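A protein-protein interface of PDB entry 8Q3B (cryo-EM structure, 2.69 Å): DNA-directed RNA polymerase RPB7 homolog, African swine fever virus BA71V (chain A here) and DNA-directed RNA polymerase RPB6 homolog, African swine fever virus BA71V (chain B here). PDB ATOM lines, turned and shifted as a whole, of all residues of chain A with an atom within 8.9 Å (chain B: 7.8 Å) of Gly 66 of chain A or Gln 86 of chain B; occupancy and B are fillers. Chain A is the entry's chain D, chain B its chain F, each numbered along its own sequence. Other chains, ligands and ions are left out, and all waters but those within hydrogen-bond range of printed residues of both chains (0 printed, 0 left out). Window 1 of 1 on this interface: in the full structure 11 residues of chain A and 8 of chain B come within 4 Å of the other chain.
The side-chain amide oxygen of Gln 86 of chain B lies within hydrogen-bond range of the side-chain hydroxyl of Thr 17 of chain A, at 3.5 Å.
O of Met 60 of chain A is in hydrogen-bond range of NH2 of Arg 78 of chain B.
The side-chain carboxylate (OD1) of Asp 14 of chain A is in salt-bridge range of the guanidinium group (NE) of Arg 67 of chain A (3.2 Å).
OD1 of Asp 15 of chain A lies within hydrogen-bond range of N of Asn 18 of chain A.
SG of Cys 20 of chain A sits close to O of Pro 16 of chain A (3.6 Å).
The side-chain sulfur of Met 60 of chain A sits at hydrogen-bond distance from the side-chain amide nitrogen of Asn 63 of chain A, at 3.3 Å.
N of Met 60 of chain A sits at hydrogen-bond distance from O of Arg 67 of chain A, 3.2 Å away.
The guanidinium group of Arg 83 of chain B is in hydrogen-bond range of the backbone carbonyl oxygen of Ser 92 of chain B, 3.3 Å away.
Among the printed residues, pairs that only touch across the chains: Asp 14 of chain A with Ile 89 of chain B, Asp 15 of chain A with Ile 89 of chain B, Asp 15 of chain A with Asn 90 of chain B, Pro 16 of chain A with Gln 86 of chain B, Thr 17 of chain A with Arg 83 of chain B, Ile 59 of chain A with Gln 86 of chain B, Arg 61 of chain A with Arg 78 of chain B, Asn 64 of chain A with Gln 85 of chain B, Gly 66 of chain A with Gln 85 of chain B and Gly 66 of chain A with Gln 86 of chain B.
Printed residues of chain A within 4 Å of Gln 86 of chain B: Pro 16 (3.9 Å), Thr 17 (3.5 Å), Ile 59 (3.3 Å) and Gly 66 (3.5 Å).
Of the printed residues of chain B, Pro 16 of chain A touches Gln 86.
Of the printed residues of chain B, Asp 15 of chain A touches Ile 89 (3.9 Å) and Asn 90 (3.5 Å).
Ala 84 of chain B touches none of the printed residues of chain A.
The nearest residue of chain B that does not touch Gly 66 of chain A is Ile 89 of chain B (4.1 Å).
Of the 19 printed residues of chain A, 9 touch a printed residue of chain B.
Printed residues of chain A that touch a printed residue of chain B: Asp 14, Asp 15, Pro 16, Thr 17, Ile 59, Met 60, Arg 61, Asn 64 and Gly 66.
Along chain A the printed residues that touch a printed residue of chain B span positions 14 to 66.
Of the 19 printed residues of chain B, 6 touch a printed residue of chain A.
Hydrophobic or aromatic side chains of chain B that line the printed part of chain A: Ile 89.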
ATOM      1  N   ILE A  13      -7.975 -21.415 -26.378  1.00  0.00           N
ATOM      2  CA  ILE A  13      -7.370 -20.271 -27.047  1.00  0.00           C
ATOM      3  C   ILE A  13      -6.108 -20.762 -27.740  1.00  0.00           C
ATOM      4  O   ILE A  13      -5.159 -21.201 -27.075  1.00  0.00           O
ATOM      5  CB  ILE A  13      -7.053 -19.139 -26.058  1.00  0.00           C
ATOM      6  CG1 ILE A  13      -8.332 -18.657 -25.374  1.00  0.00           C
ATOM      7  CG2 ILE A  13      -6.381 -17.978 -26.769  1.00  0.00           C
ATOM      8  CD1 ILE A  13      -8.112 -18.143 -23.977  1.00  0.00           C
ATOM      9  N   ASP A  14      -6.100 -20.691 -29.072  1.00  0.00           N
ATOM     10  CA  ASP A  14      -4.975 -21.204 -29.844  1.00  0.00           C
ATOM     11  C   ASP A  14      -3.776 -20.264 -29.820  1.00  0.00           C
ATOM     12  O   ASP A  14      -2.633 -20.729 -29.885  1.00  0.00           O
ATOM     13  CB  ASP A  14      -5.408 -21.456 -31.289  1.00  0.00           C
ATOM     14  CG  ASP A  14      -6.678 -22.274 -31.381  1.00  0.00           C
ATOM     15  OD1 ASP A  14      -6.679 -23.429 -30.904  1.00  0.00           O
ATOM     16  OD2 ASP A  14      -7.677 -21.764 -31.928  1.00  0.00           O
ATOM     17  N   ASP A  15      -4.009 -18.956 -29.730  1.00  0.00           N
ATOM     18  CA  ASP A  15      -2.946 -17.952 -29.737  1.00  0.00           C
ATOM     19  C   ASP A  15      -3.153 -17.034 -28.541  1.00  0.00           C
ATOM     20  O   ASP A  15      -3.678 -15.921 -28.680  1.00  0.00           O
ATOM     21  CB  ASP A  15      -2.940 -17.166 -31.049  1.00  0.00           C
ATOM     22  CG  ASP A  15      -1.800 -16.171 -31.126  1.00  0.00           C
ATOM     23  OD1 ASP A  15      -0.927 -16.194 -30.234  1.00  0.00           O
ATOM     24  OD2 ASP A  15      -1.773 -15.370 -32.083  1.00  0.00           O
ATOM     25  N   PRO A  16      -2.753 -17.472 -27.343  1.00  0.00           N
ATOM     26  CA  PRO A  16      -3.011 -16.647 -26.148  1.00  0.00           C
ATOM     27  C   PRO A  16      -2.404 -15.258 -26.223  1.00  0.00           C
ATOM     28  O   PRO A  16      -3.013 -14.294 -25.743  1.00  0.00           O
ATOM     29  CB  PRO A  16      -2.392 -17.477 -25.015  1.00  0.00           C
ATOM     30  CG  PRO A  16      -2.321 -18.868 -25.542  1.00  0.00           C
ATOM     31  CD  PRO A  16      -2.080 -18.736 -27.008  1.00  0.00           C
ATOM     32  N   THR A  17      -1.213 -15.124 -26.813  1.00  0.00           N
ATOM     33  CA  THR A  17      -0.565 -13.817 -26.867  1.00  0.00           C
ATOM     34  C   THR A  17      -1.414 -12.815 -27.639  1.00  0.00           C
ATOM     35  O   THR A  17      -1.591 -11.674 -27.201  1.00  0.00           O
ATOM     36  CB  THR A  17       0.820 -13.945 -27.502  1.00  0.00           C
ATOM     37  OG1 THR A  17       1.592 -14.913 -26.782  1.00  0.00           O
ATOM     38  CG2 THR A  17       1.547 -12.607 -27.479  1.00  0.00           C
ATOM     39  N   ASN A  18      -1.945 -13.224 -28.792  1.00  0.00           N
ATOM     40  CA  ASN A  18      -2.826 -12.343 -29.549  1.00  0.00           C
ATOM     41  C   ASN A  18      -4.187 -12.209 -28.882  1.00  0.00           C
ATOM     42  O   ASN A  18      -4.806 -11.141 -28.946  1.00  0.00           O
ATOM     43  CB  ASN A  18      -2.990 -12.864 -30.974  1.00  0.00           C
ATOM     44  CG  ASN A  18      -4.039 -12.102 -31.754  1.00  0.00           C
ATOM     45  OD1 ASN A  18      -4.188 -10.891 -31.599  1.00  0.00           O
ATOM     46  ND2 ASN A  18      -4.777 -12.810 -32.601  1.00  0.00           N
ATOM     47  N   CYS A  20      -4.961 -12.127 -25.687  1.00  0.00           N
ATOM     48  CA  CYS A  20      -4.971 -11.272 -24.505  1.00  0.00           C
ATOM     49  C   CYS A  20      -4.874  -9.788 -24.832  1.00  0.00           C
ATOM     50  O   CYS A  20      -5.035  -8.966 -23.925  1.00  0.00           O
ATOM     51  CB  CYS A  20      -3.829 -11.660 -23.569  1.00  0.00           C
ATOM     52  SG  CYS A  20      -4.181 -13.106 -22.552  1.00  0.00           S
ATOM     53  N   CYS A  57      -6.254 -16.410 -18.340  1.00  0.00           N
ATOM     54  CA  CYS A  57      -5.975 -17.273 -19.480  1.00  0.00           C
ATOM     55  C   CYS A  57      -4.904 -18.292 -19.115  1.00  0.00           C
ATOM     56  O   CYS A  57      -3.712 -18.059 -19.338  1.00  0.00           O
ATOM     57  CB  CYS A  57      -5.534 -16.444 -20.687  1.00  0.00           C
ATOM     58  SG  CYS A  57      -5.312 -17.405 -22.200  1.00  0.00           S
ATOM     59  N   PHE A  58      -5.323 -19.422 -18.554  1.00  0.00           N
ATOM     60  CA  PHE A  58      -4.387 -20.453 -18.142  1.00  0.00           C
ATOM     61  C   PHE A  58      -3.692 -21.061 -19.359  1.00  0.00           C
ATOM     62  O   PHE A  58      -4.050 -20.804 -20.511  1.00  0.00           O
ATOM     63  CB  PHE A  58      -5.108 -21.542 -17.352  1.00  0.00           C
ATOM     64  CG  PHE A  58      -5.789 -21.043 -16.111  1.00  0.00           C
ATOM     65  CD1 PHE A  58      -5.052 -20.697 -14.993  1.00  0.00           C
ATOM     66  CD2 PHE A  58      -7.166 -20.924 -16.061  1.00  0.00           C
ATOM     67  CE1 PHE A  58      -5.676 -20.240 -13.851  1.00  0.00           C
ATOM     68  CE2 PHE A  58      -7.793 -20.467 -14.920  1.00  0.00           C
ATOM     69  CZ  PHE A  58      -7.048 -20.126 -13.814  1.00  0.00           C
ATOM     70  N   ILE A  59      -2.681 -21.880 -19.085  1.00  0.00           N
ATOM     71  CA  ILE A  59      -1.922 -22.588 -20.109  1.00  0.00           C
ATOM     72  C   ILE A  59      -2.109 -24.081 -19.885  1.00  0.00           C
ATOM     73  O   ILE A  59      -1.953 -24.568 -18.758  1.00  0.00           O
ATOM     74  CB  ILE A  59      -0.430 -22.210 -20.073  1.00  0.00           C
ATOM     75  CG1 ILE A  59      -0.252 -20.693 -20.188  1.00  0.00           C
ATOM     76  CG2 ILE A  59       0.326 -22.916 -21.187  1.00  0.00           C
ATOM     77  CD1 ILE A  59      -0.838 -20.085 -21.443  1.00  0.00           C
ATOM     78  N   MET A  60      -2.444 -24.802 -20.951  1.00  0.00           N
ATOM     79  CA  MET A  60      -2.728 -26.227 -20.836  1.00  0.00           C
ATOM     80  C   MET A  60      -1.497 -26.984 -20.354  1.00  0.00           C
ATOM     81  O   MET A  60      -0.433 -26.923 -20.978  1.00  0.00           O
ATOM     82  CB  MET A  60      -3.195 -26.774 -22.183  1.00  0.00           C
ATOM     83  CG  MET A  60      -4.351 -26.004 -22.797  1.00  0.00           C
ATOM     84  SD  MET A  60      -5.222 -26.947 -24.059  1.00  0.00           S
ATOM     85  CE  MET A  60      -6.103 -25.642 -24.907  1.00  0.00           C
ATOM     86  N   ARG A  61      -1.650 -27.700 -19.238  1.00  0.00           N
ATOM     87  CA  ARG A  61      -0.550 -28.498 -18.703  1.00  0.00           C
ATOM     88  C   ARG A  61      -0.387 -29.805 -19.468  1.00  0.00           C
ATOM     89  O   ARG A  61       0.728 -30.181 -19.846  1.00  0.00           O
ATOM     90  CB  ARG A  61      -0.791 -28.793 -17.224  1.00  0.00           C
ATOM     91  CG  ARG A  61      -0.494 -27.650 -16.276  1.00  0.00           C
ATOM     92  CD  ARG A  61      -0.477 -28.150 -14.840  1.00  0.00           C
ATOM     93  NE  ARG A  61      -1.464 -29.205 -14.626  1.00  0.00           N
ATOM     94  CZ  ARG A  61      -1.188 -30.497 -14.496  1.00  0.00           C
ATOM     95  NH1 ARG A  61       0.050 -30.957 -14.580  1.00  0.00           N
ATOM     96  NH2 ARG A  61      -2.182 -31.354 -14.287  1.00  0.00           N
ATOM     97  N   ASN A  63      -1.038 -31.093 -22.418  1.00  0.00           N
ATOM     98  CA  ASN A  63      -0.436 -31.105 -23.742  1.00  0.00           C
ATOM     99  C   ASN A  63       0.756 -30.157 -23.790  1.00  0.00           C
ATOM    100  O   ASN A  63       0.893 -29.248 -22.969  1.00  0.00           O
ATOM    101  CB  ASN A  63      -1.456 -30.726 -24.819  1.00  0.00           C
ATOM    102  CG  ASN A  63      -2.253 -29.491 -24.466  1.00  0.00           C
ATOM    103  OD1 ASN A  63      -1.856 -28.371 -24.783  1.00  0.00           O
ATOM    104  ND2 ASN A  63      -3.391 -29.690 -23.815  1.00  0.00           N
ATOM    105  N   ASN A  64       1.622 -30.384 -24.772  1.00  0.00           N
ATOM    106  CA  ASN A  64       2.852 -29.620 -24.924  1.00  0.00           C
ATOM    107  C   ASN A  64       2.687 -28.410 -25.832  1.00  0.00           C
ATOM    108  O   ASN A  64       3.684 -27.764 -26.170  1.00  0.00           O
ATOM    109  CB  ASN A  64       3.967 -30.523 -25.464  1.00  0.00           C
ATOM    110  CG  ASN A  64       4.937 -30.967 -24.383  1.00  0.00           C
ATOM    111  OD1 ASN A  64       4.798 -30.605 -23.217  1.00  0.00           O
ATOM    112  ND2 ASN A  64       5.928 -31.756 -24.774  1.00  0.00           N
ATOM    113  N   SER A  65       1.464 -28.096 -26.243  1.00  0.00           N
ATOM    114  CA  SER A  65       1.210 -26.887 -27.008  1.00  0.00           C
ATOM    115  C   SER A  65       1.080 -25.690 -26.077  1.00  0.00           C
ATOM    116  O   SER A  65       0.666 -25.815 -24.920  1.00  0.00           O
ATOM    117  CB  SER A  65      -0.063 -27.037 -27.840  1.00  0.00           C
ATOM    118  OG  SER A  65      -1.184 -27.267 -27.006  1.00  0.00           O
ATOM    119  N   GLY A  66       1.439 -24.515 -26.592  1.00  0.00           N
ATOM    120  CA  GLY A  66       1.304 -23.294 -25.821  1.00  0.00           C
ATOM    121  C   GLY A  66      -0.120 -22.803 -25.679  1.00  0.00           C
ATOM    122  O   GLY A  66      -0.345 -21.801 -24.994  1.00  0.00           O
ATOM    123  N   ARG A  67      -1.076 -23.482 -26.311  1.00  0.00           N
ATOM    124  CA  ARG A  67      -2.473 -23.075 -26.242  1.00  0.00           C
ATOM    125  C   ARG A  67      -2.911 -22.919 -24.792  1.00  0.00           C
ATOM    126  O   ARG A  67      -2.382 -23.570 -23.888  1.00  0.00           O
ATOM    127  CB  ARG A  67      -3.352 -24.108 -26.950  1.00  0.00           C
ATOM    128  CG  ARG A  67      -2.974 -24.347 -28.404  1.00  0.00           C
ATOM    129  CD  ARG A  67      -3.663 -25.572 -28.977  1.00  0.00           C
ATOM    130  NE  ARG A  67      -5.118 -25.454 -28.950  1.00  0.00           N
ATOM    131  CZ  ARG A  67      -5.948 -26.343 -28.417  1.00  0.00           C
ATOM    132  NH1 ARG A  67      -5.507 -27.454 -27.845  1.00  0.00           N
ATOM    133  NH2 ARG A  67      -7.256 -26.114 -28.462  1.00  0.00           N
ATOM    134  N   GLY A  68      -3.883 -22.033 -24.573  1.00  0.00           N
ATOM    135  CA  GLY A  68      -4.436 -21.792 -23.261  1.00  0.00           C
ATOM    136  C   GLY A  68      -5.918 -22.120 -23.208  1.00  0.00           C
ATOM    137  O   GLY A  68      -6.520 -22.555 -24.191  1.00  0.00           O
ATOM    138  N   TYR A  69      -6.499 -21.895 -22.033  1.00  0.00           N
ATOM    139  CA  TYR A  69      -7.931 -22.071 -21.862  1.00  0.00           C
ATOM    140  C   TYR A  69      -8.439 -21.045 -20.863  1.00  0.00           C
ATOM    141  O   TYR A  69      -7.695 -20.555 -20.011  1.00  0.00           O
ATOM    142  CB  TYR A  69      -8.281 -23.492 -21.404  1.00  0.00           C
ATOM    143  CG  TYR A  69      -7.679 -23.886 -20.077  1.00  0.00           C
ATOM    144  CD1 TYR A  69      -6.352 -24.272 -19.983  1.00  0.00           C
ATOM    145  CD2 TYR A  69      -8.443 -23.880 -18.920  1.00  0.00           C
ATOM    146  CE1 TYR A  69      -5.801 -24.636 -18.774  1.00  0.00           C
ATOM    147  CE2 TYR A  69      -7.899 -24.242 -17.707  1.00  0.00           C
ATOM    148  CZ  TYR A  69      -6.578 -24.620 -17.639  1.00  0.00           C
ATOM    149  OH  TYR A  69      -6.029 -24.982 -16.432  1.00  0.00           O
ATOM    150  N   ARG B  78       9.645 -23.781 -16.787  1.00  0.00           N
ATOM    151  CA  ARG B  78       8.290 -23.797 -17.327  1.00  0.00           C
ATOM    152  C   ARG B  78       7.964 -22.485 -18.028  1.00  0.00           C
ATOM    153  O   ARG B  78       7.363 -22.483 -19.109  1.00  0.00           O
ATOM    154  CB  ARG B  78       7.288 -24.076 -16.205  1.00  0.00           C
ATOM    155  CG  ARG B  78       5.828 -23.991 -16.618  1.00  0.00           C
ATOM    156  CD  ARG B  78       5.420 -25.171 -17.479  1.00  0.00           C
ATOM    157  NE  ARG B  78       3.988 -25.172 -17.749  1.00  0.00           N
ATOM    158  CZ  ARG B  78       3.413 -25.812 -18.758  1.00  0.00           C
ATOM    159  NH1 ARG B  78       4.120 -26.529 -19.615  1.00  0.00           N
ATOM    160  NH2 ARG B  78       2.095 -25.731 -18.910  1.00  0.00           N
ATOM    161  N   LEU B  79       8.344 -21.358 -17.425  1.00  0.00           N
ATOM    162  CA  LEU B  79       8.092 -20.065 -18.050  1.00  0.00           C
ATOM    163  C   LEU B  79       8.791 -19.972 -19.397  1.00  0.00           C
ATOM    164  O   LEU B  79       8.189 -19.564 -20.398  1.00  0.00           O
ATOM    165  CB  LEU B  79       8.560 -18.938 -17.130  1.00  0.00           C
ATOM    166  CG  LEU B  79       7.606 -18.497 -16.021  1.00  0.00           C
ATOM    167  CD1 LEU B  79       8.328 -17.578 -15.056  1.00  0.00           C
ATOM    168  CD2 LEU B  79       6.386 -17.805 -16.599  1.00  0.00           C
ATOM    169  N   VAL B  80      10.069 -20.357 -19.444  1.00  0.00           N
ATOM    170  CA  VAL B  80      10.817 -20.265 -20.694  1.00  0.00           C
ATOM    171  C   VAL B  80      10.203 -21.177 -21.746  1.00  0.00           C
ATOM    172  O   VAL B  80      10.069 -20.795 -22.912  1.00  0.00           O
ATOM    173  CB  VAL B  80      12.303 -20.591 -20.454  1.00  0.00           C
ATOM    174  CG1 VAL B  80      13.056 -20.666 -21.774  1.00  0.00           C
ATOM    175  CG2 VAL B  80      12.932 -19.550 -19.550  1.00  0.00           C
ATOM    176  N   ALA B  81       9.821 -22.395 -21.357  1.00  0.00           N
ATOM    177  CA  ALA B  81       9.256 -23.337 -22.318  1.00  0.00           C
ATOM    178  C   ALA B  81       7.934 -22.829 -22.877  1.00  0.00           C
ATOM    179  O   ALA B  81       7.693 -22.885 -24.090  1.00  0.00           O
ATOM    180  CB  ALA B  81       9.071 -24.702 -21.657  1.00  0.00           C
ATOM    181  N   VAL B  82       7.055 -22.333 -22.004  1.00  0.00           N
ATOM    182  CA  VAL B  82       5.764 -21.831 -22.463  1.00  0.00           C
ATOM    183  C   VAL B  82       5.961 -20.631 -23.377  1.00  0.00           C
ATOM    184  O   VAL B  82       5.303 -20.513 -24.420  1.00  0.00           O
ATOM    185  CB  VAL B  82       4.866 -21.485 -21.262  1.00  0.00           C
ATOM    186  CG1 VAL B  82       3.703 -20.611 -21.700  1.00  0.00           C
ATOM    187  CG2 VAL B  82       4.362 -22.754 -20.599  1.00  0.00           C
ATOM    188  N   ARG B  83       6.863 -19.721 -23.005  1.00  0.00           N
ATOM    189  CA  ARG B  83       7.095 -18.552 -23.842  1.00  0.00           C
ATOM    190  C   ARG B  83       7.678 -18.949 -25.191  1.00  0.00           C
ATOM    191  O   ARG B  83       7.330 -18.363 -26.219  1.00  0.00           O
ATOM    192  CB  ARG B  83       8.017 -17.562 -23.130  1.00  0.00           C
ATOM    193  CG  ARG B  83       8.245 -16.260 -23.892  1.00  0.00           C
ATOM    194  CD  ARG B  83       6.935 -15.574 -24.260  1.00  0.00           C
ATOM    195  NE  ARG B  83       7.149 -14.335 -24.998  1.00  0.00           N
ATOM    196  CZ  ARG B  83       6.336 -13.865 -25.936  1.00  0.00           C
ATOM    197  NH1 ARG B  83       5.221 -14.495 -26.267  1.00  0.00           N
ATOM    198  NH2 ARG B  83       6.648 -12.731 -26.554  1.00  0.00           N
ATOM    199  N   ALA B  84       8.572 -19.941 -25.210  1.00  0.00           N
ATOM    200  CA  ALA B  84       9.135 -20.398 -26.475  1.00  0.00           C
ATOM    201  C   ALA B  84       8.063 -21.011 -27.365  1.00  0.00           C
ATOM    202  O   ALA B  84       8.033 -20.763 -28.577  1.00  0.00           O
ATOM    203  CB  ALA B  84      10.255 -21.405 -26.214  1.00  0.00           C
ATOM    204  N   GLN B  85       7.172 -21.818 -26.786  1.00  0.00           N
ATOM    205  CA  GLN B  85       6.094 -22.397 -27.584  1.00  0.00           C
ATOM    206  C   GLN B  85       5.178 -21.312 -28.138  1.00  0.00           C
ATOM    207  O   GLN B  85       4.790 -21.353 -29.313  1.00  0.00           O
ATOM    208  CB  GLN B  85       5.295 -23.396 -26.749  1.00  0.00           C
ATOM    209  CG  GLN B  85       5.402 -24.834 -27.232  1.00  0.00           C
ATOM    210  CD  GLN B  85       4.998 -24.996 -28.685  1.00  0.00           C
ATOM    211  OE1 GLN B  85       4.295 -24.156 -29.243  1.00  0.00           O
ATOM    212  NE2 GLN B  85       5.444 -26.082 -29.304  1.00  0.00           N
ATOM    213  N   GLN B  86       4.826 -20.326 -27.310  1.00  0.00           N
ATOM    214  CA  GLN B  86       3.964 -19.253 -27.790  1.00  0.00           C
ATOM    215  C   GLN B  86       4.665 -18.394 -28.834  1.00  0.00           C
ATOM    216  O   GLN B  86       4.011 -17.864 -29.738  1.00  0.00           O
ATOM    217  CB  GLN B  86       3.491 -18.402 -26.613  1.00  0.00           C
ATOM    218  CG  GLN B  86       2.605 -19.167 -25.645  1.00  0.00           C
ATOM    219  CD  GLN B  86       2.107 -18.312 -24.504  1.00  0.00           C
ATOM    220  OE1 GLN B  86       2.561 -17.185 -24.310  1.00  0.00           O
ATOM    221  NE2 GLN B  86       1.162 -18.843 -23.737  1.00  0.00           N
ATOM    222  N   LEU B  87       5.986 -18.240 -28.726  1.00  0.00           N
ATOM    223  CA  LEU B  87       6.742 -17.565 -29.776  1.00  0.00           C
ATOM    224  C   LEU B  87       6.684 -18.355 -31.074  1.00  0.00           C
ATOM    225  O   LEU B  87       6.540 -17.778 -32.158  1.00  0.00           O
ATOM    226  CB  LEU B  87       8.191 -17.370 -29.336  1.00  0.00           C
ATOM    227  CG  LEU B  87       8.459 -16.106 -28.521  1.00  0.00           C
ATOM    228  CD1 LEU B  87       9.739 -16.251 -27.725  1.00  0.00           C
ATOM    229  CD2 LEU B  87       8.529 -14.895 -29.431  1.00  0.00           C
ATOM    230  N   ALA B  88       6.801 -19.681 -30.984  1.00  0.00           N
ATOM    231  CA  ALA B  88       6.631 -20.516 -32.165  1.00  0.00           C
ATOM    232  C   ALA B  88       5.248 -20.324 -32.769  1.00  0.00           C
ATOM    233  O   ALA B  88       5.086 -20.354 -33.995  1.00  0.00           O
ATOM    234  CB  ALA B  88       6.864 -21.984 -31.810  1.00  0.00           C
ATOM    235  N   ILE B  89       4.236 -20.125 -31.924  1.00  0.00           N
ATOM    236  CA  ILE B  89       2.892 -19.858 -32.431  1.00  0.00           C
ATOM    237  C   ILE B  89       2.813 -18.451 -33.016  1.00  0.00           C
ATOM    238  O   ILE B  89       2.417 -18.263 -34.171  1.00  0.00           O
ATOM    239  CB  ILE B  89       1.847 -20.063 -31.319  1.00  0.00           C
ATOM    240  CG1 ILE B  89       1.744 -21.546 -30.960  1.00  0.00           C
ATOM    241  CG2 ILE B  89       0.490 -19.523 -31.756  1.00  0.00           C
ATOM    242  CD1 ILE B  89       0.941 -21.824 -29.705  1.00  0.00           C
ATOM    243  N   ASN B  90       3.189 -17.444 -32.228  1.00  0.00           N
ATOM    244  CA  ASN B  90       3.143 -16.047 -32.647  1.00  0.00           C
ATOM    245  C   ASN B  90       4.517 -15.434 -32.437  1.00  0.00           C
ATOM    246  O   ASN B  90       5.037 -15.445 -31.317  1.00  0.00           O
ATOM    247  CB  ASN B  90       2.082 -15.274 -31.860  1.00  0.00           C
ATOM    248  CG  ASN B  90       1.934 -13.843 -32.331  1.00  0.00           C
ATOM    249  OD1 ASN B  90       2.489 -13.456 -33.360  1.00  0.00           O
ATOM    250  ND2 ASN B  90       1.184 -13.047 -31.580  1.00  0.00           N
ATOM    251  N   GLY B  91       5.093 -14.883 -33.501  1.00  0.00           N
ATOM    252  CA  GLY B  91       6.465 -14.418 -33.477  1.00  0.00           C
ATOM    253  C   GLY B  91       6.699 -13.040 -32.901  1.00  0.00           C
ATOM    254  O   GLY B  91       7.848 -12.591 -32.869  1.00  0.00           O
ATOM    255  N   SER B  92       5.660 -12.350 -32.440  1.00  0.00           N
ATOM    256  CA  SER B  92       5.834 -11.005 -31.902  1.00  0.00           C
ATOM    257  C   SER B  92       6.575 -11.071 -30.572  1.00  0.00           C
ATOM    258  O   SER B  92       6.149 -11.776 -29.651  1.00  0.00           O
ATOM    259  CB  SER B  92       4.478 -10.328 -31.727  1.00  0.00           C
ATOM    260  OG  SER B  92       4.005 -10.474 -30.401  1.00  0.00           O
ATOM    261  N   PRO B 102      13.301 -19.606 -31.084  1.00  0.00           N
ATOM    262  CA  PRO B 102      12.381 -19.217 -30.004  1.00  0.00           C
ATOM    263  C   PRO B 102      12.955 -19.435 -28.618  1.00  0.00           C
ATOM    264  O   PRO B 102      12.647 -18.666 -27.699  1.00  0.00           O
ATOM    265  CB  PRO B 102      11.153 -20.103 -30.257  1.00  0.00           C
ATOM    266  CG  PRO B 102      11.680 -21.278 -30.987  1.00  0.00           C
ATOM    267  CD  PRO B 102      12.802 -20.770 -31.838  1.00  0.00           C
ATOM    268  N   ILE B 115       9.274 -10.990 -20.010  1.00  0.00           N
ATOM    269  CA  ILE B 115       8.407 -12.142 -20.286  1.00  0.00           C
ATOM    270  C   ILE B 115       6.962 -11.774 -19.959  1.00  0.00           C
ATOM    271  O   ILE B 115       6.695 -11.227 -18.875  1.00  0.00           O
ATOM    272  CB  ILE B 115       8.871 -13.358 -19.480  1.00  0.00           C
ATOM    273  CG1 ILE B 115       8.216 -14.633 -20.010  1.00  0.00           C
ATOM    274  CG2 ILE B 115       8.572 -13.174 -18.001  1.00  0.00           C
ATOM    275  CD1 ILE B 115       8.943 -15.891 -19.608  1.00  0.00           C
ATOM    276  N   PRO B 116       5.998 -12.041 -20.852  1.00  0.00           N
ATOM    277  CA  PRO B 116       4.624 -11.577 -20.618  1.00  0.00           C
ATOM    278  C   PRO B 116       3.756 -12.548 -19.832  1.00  0.00           C
ATOM    279  O   PRO B 116       2.527 -12.425 -19.853  1.00  0.00           O
ATOM    280  CB  PRO B 116       4.090 -11.390 -22.040  1.00  0.00           C
ATOM    281  CG  PRO B 116       4.776 -12.459 -22.818  1.00  0.00           C
ATOM    282  CD  PRO B 116       6.133 -12.671 -22.178  1.00  0.00           C
ATOM    283  N   LEU B 117       4.357 -13.517 -19.153  1.00  0.00           N
ATOM    284  CA  LEU B 117       3.613 -14.520 -18.407  1.00  0.00           C
ATOM    285  C   LEU B 117       3.679 -14.238 -16.911  1.00  0.00           C
ATOM    286  O   LEU B 117       4.548 -13.507 -16.428  1.00  0.00           O
ATOM    287  CB  LEU B 117       4.148 -15.929 -18.689  1.00  0.00           C
ATOM    288  CG  LEU B 117       4.424 -16.275 -20.153  1.00  0.00           C
ATOM    289  CD1 LEU B 117       5.299 -17.511 -20.247  1.00  0.00           C
ATOM    290  CD2 LEU B 117       3.124 -16.479 -20.907  1.00  0.00           C
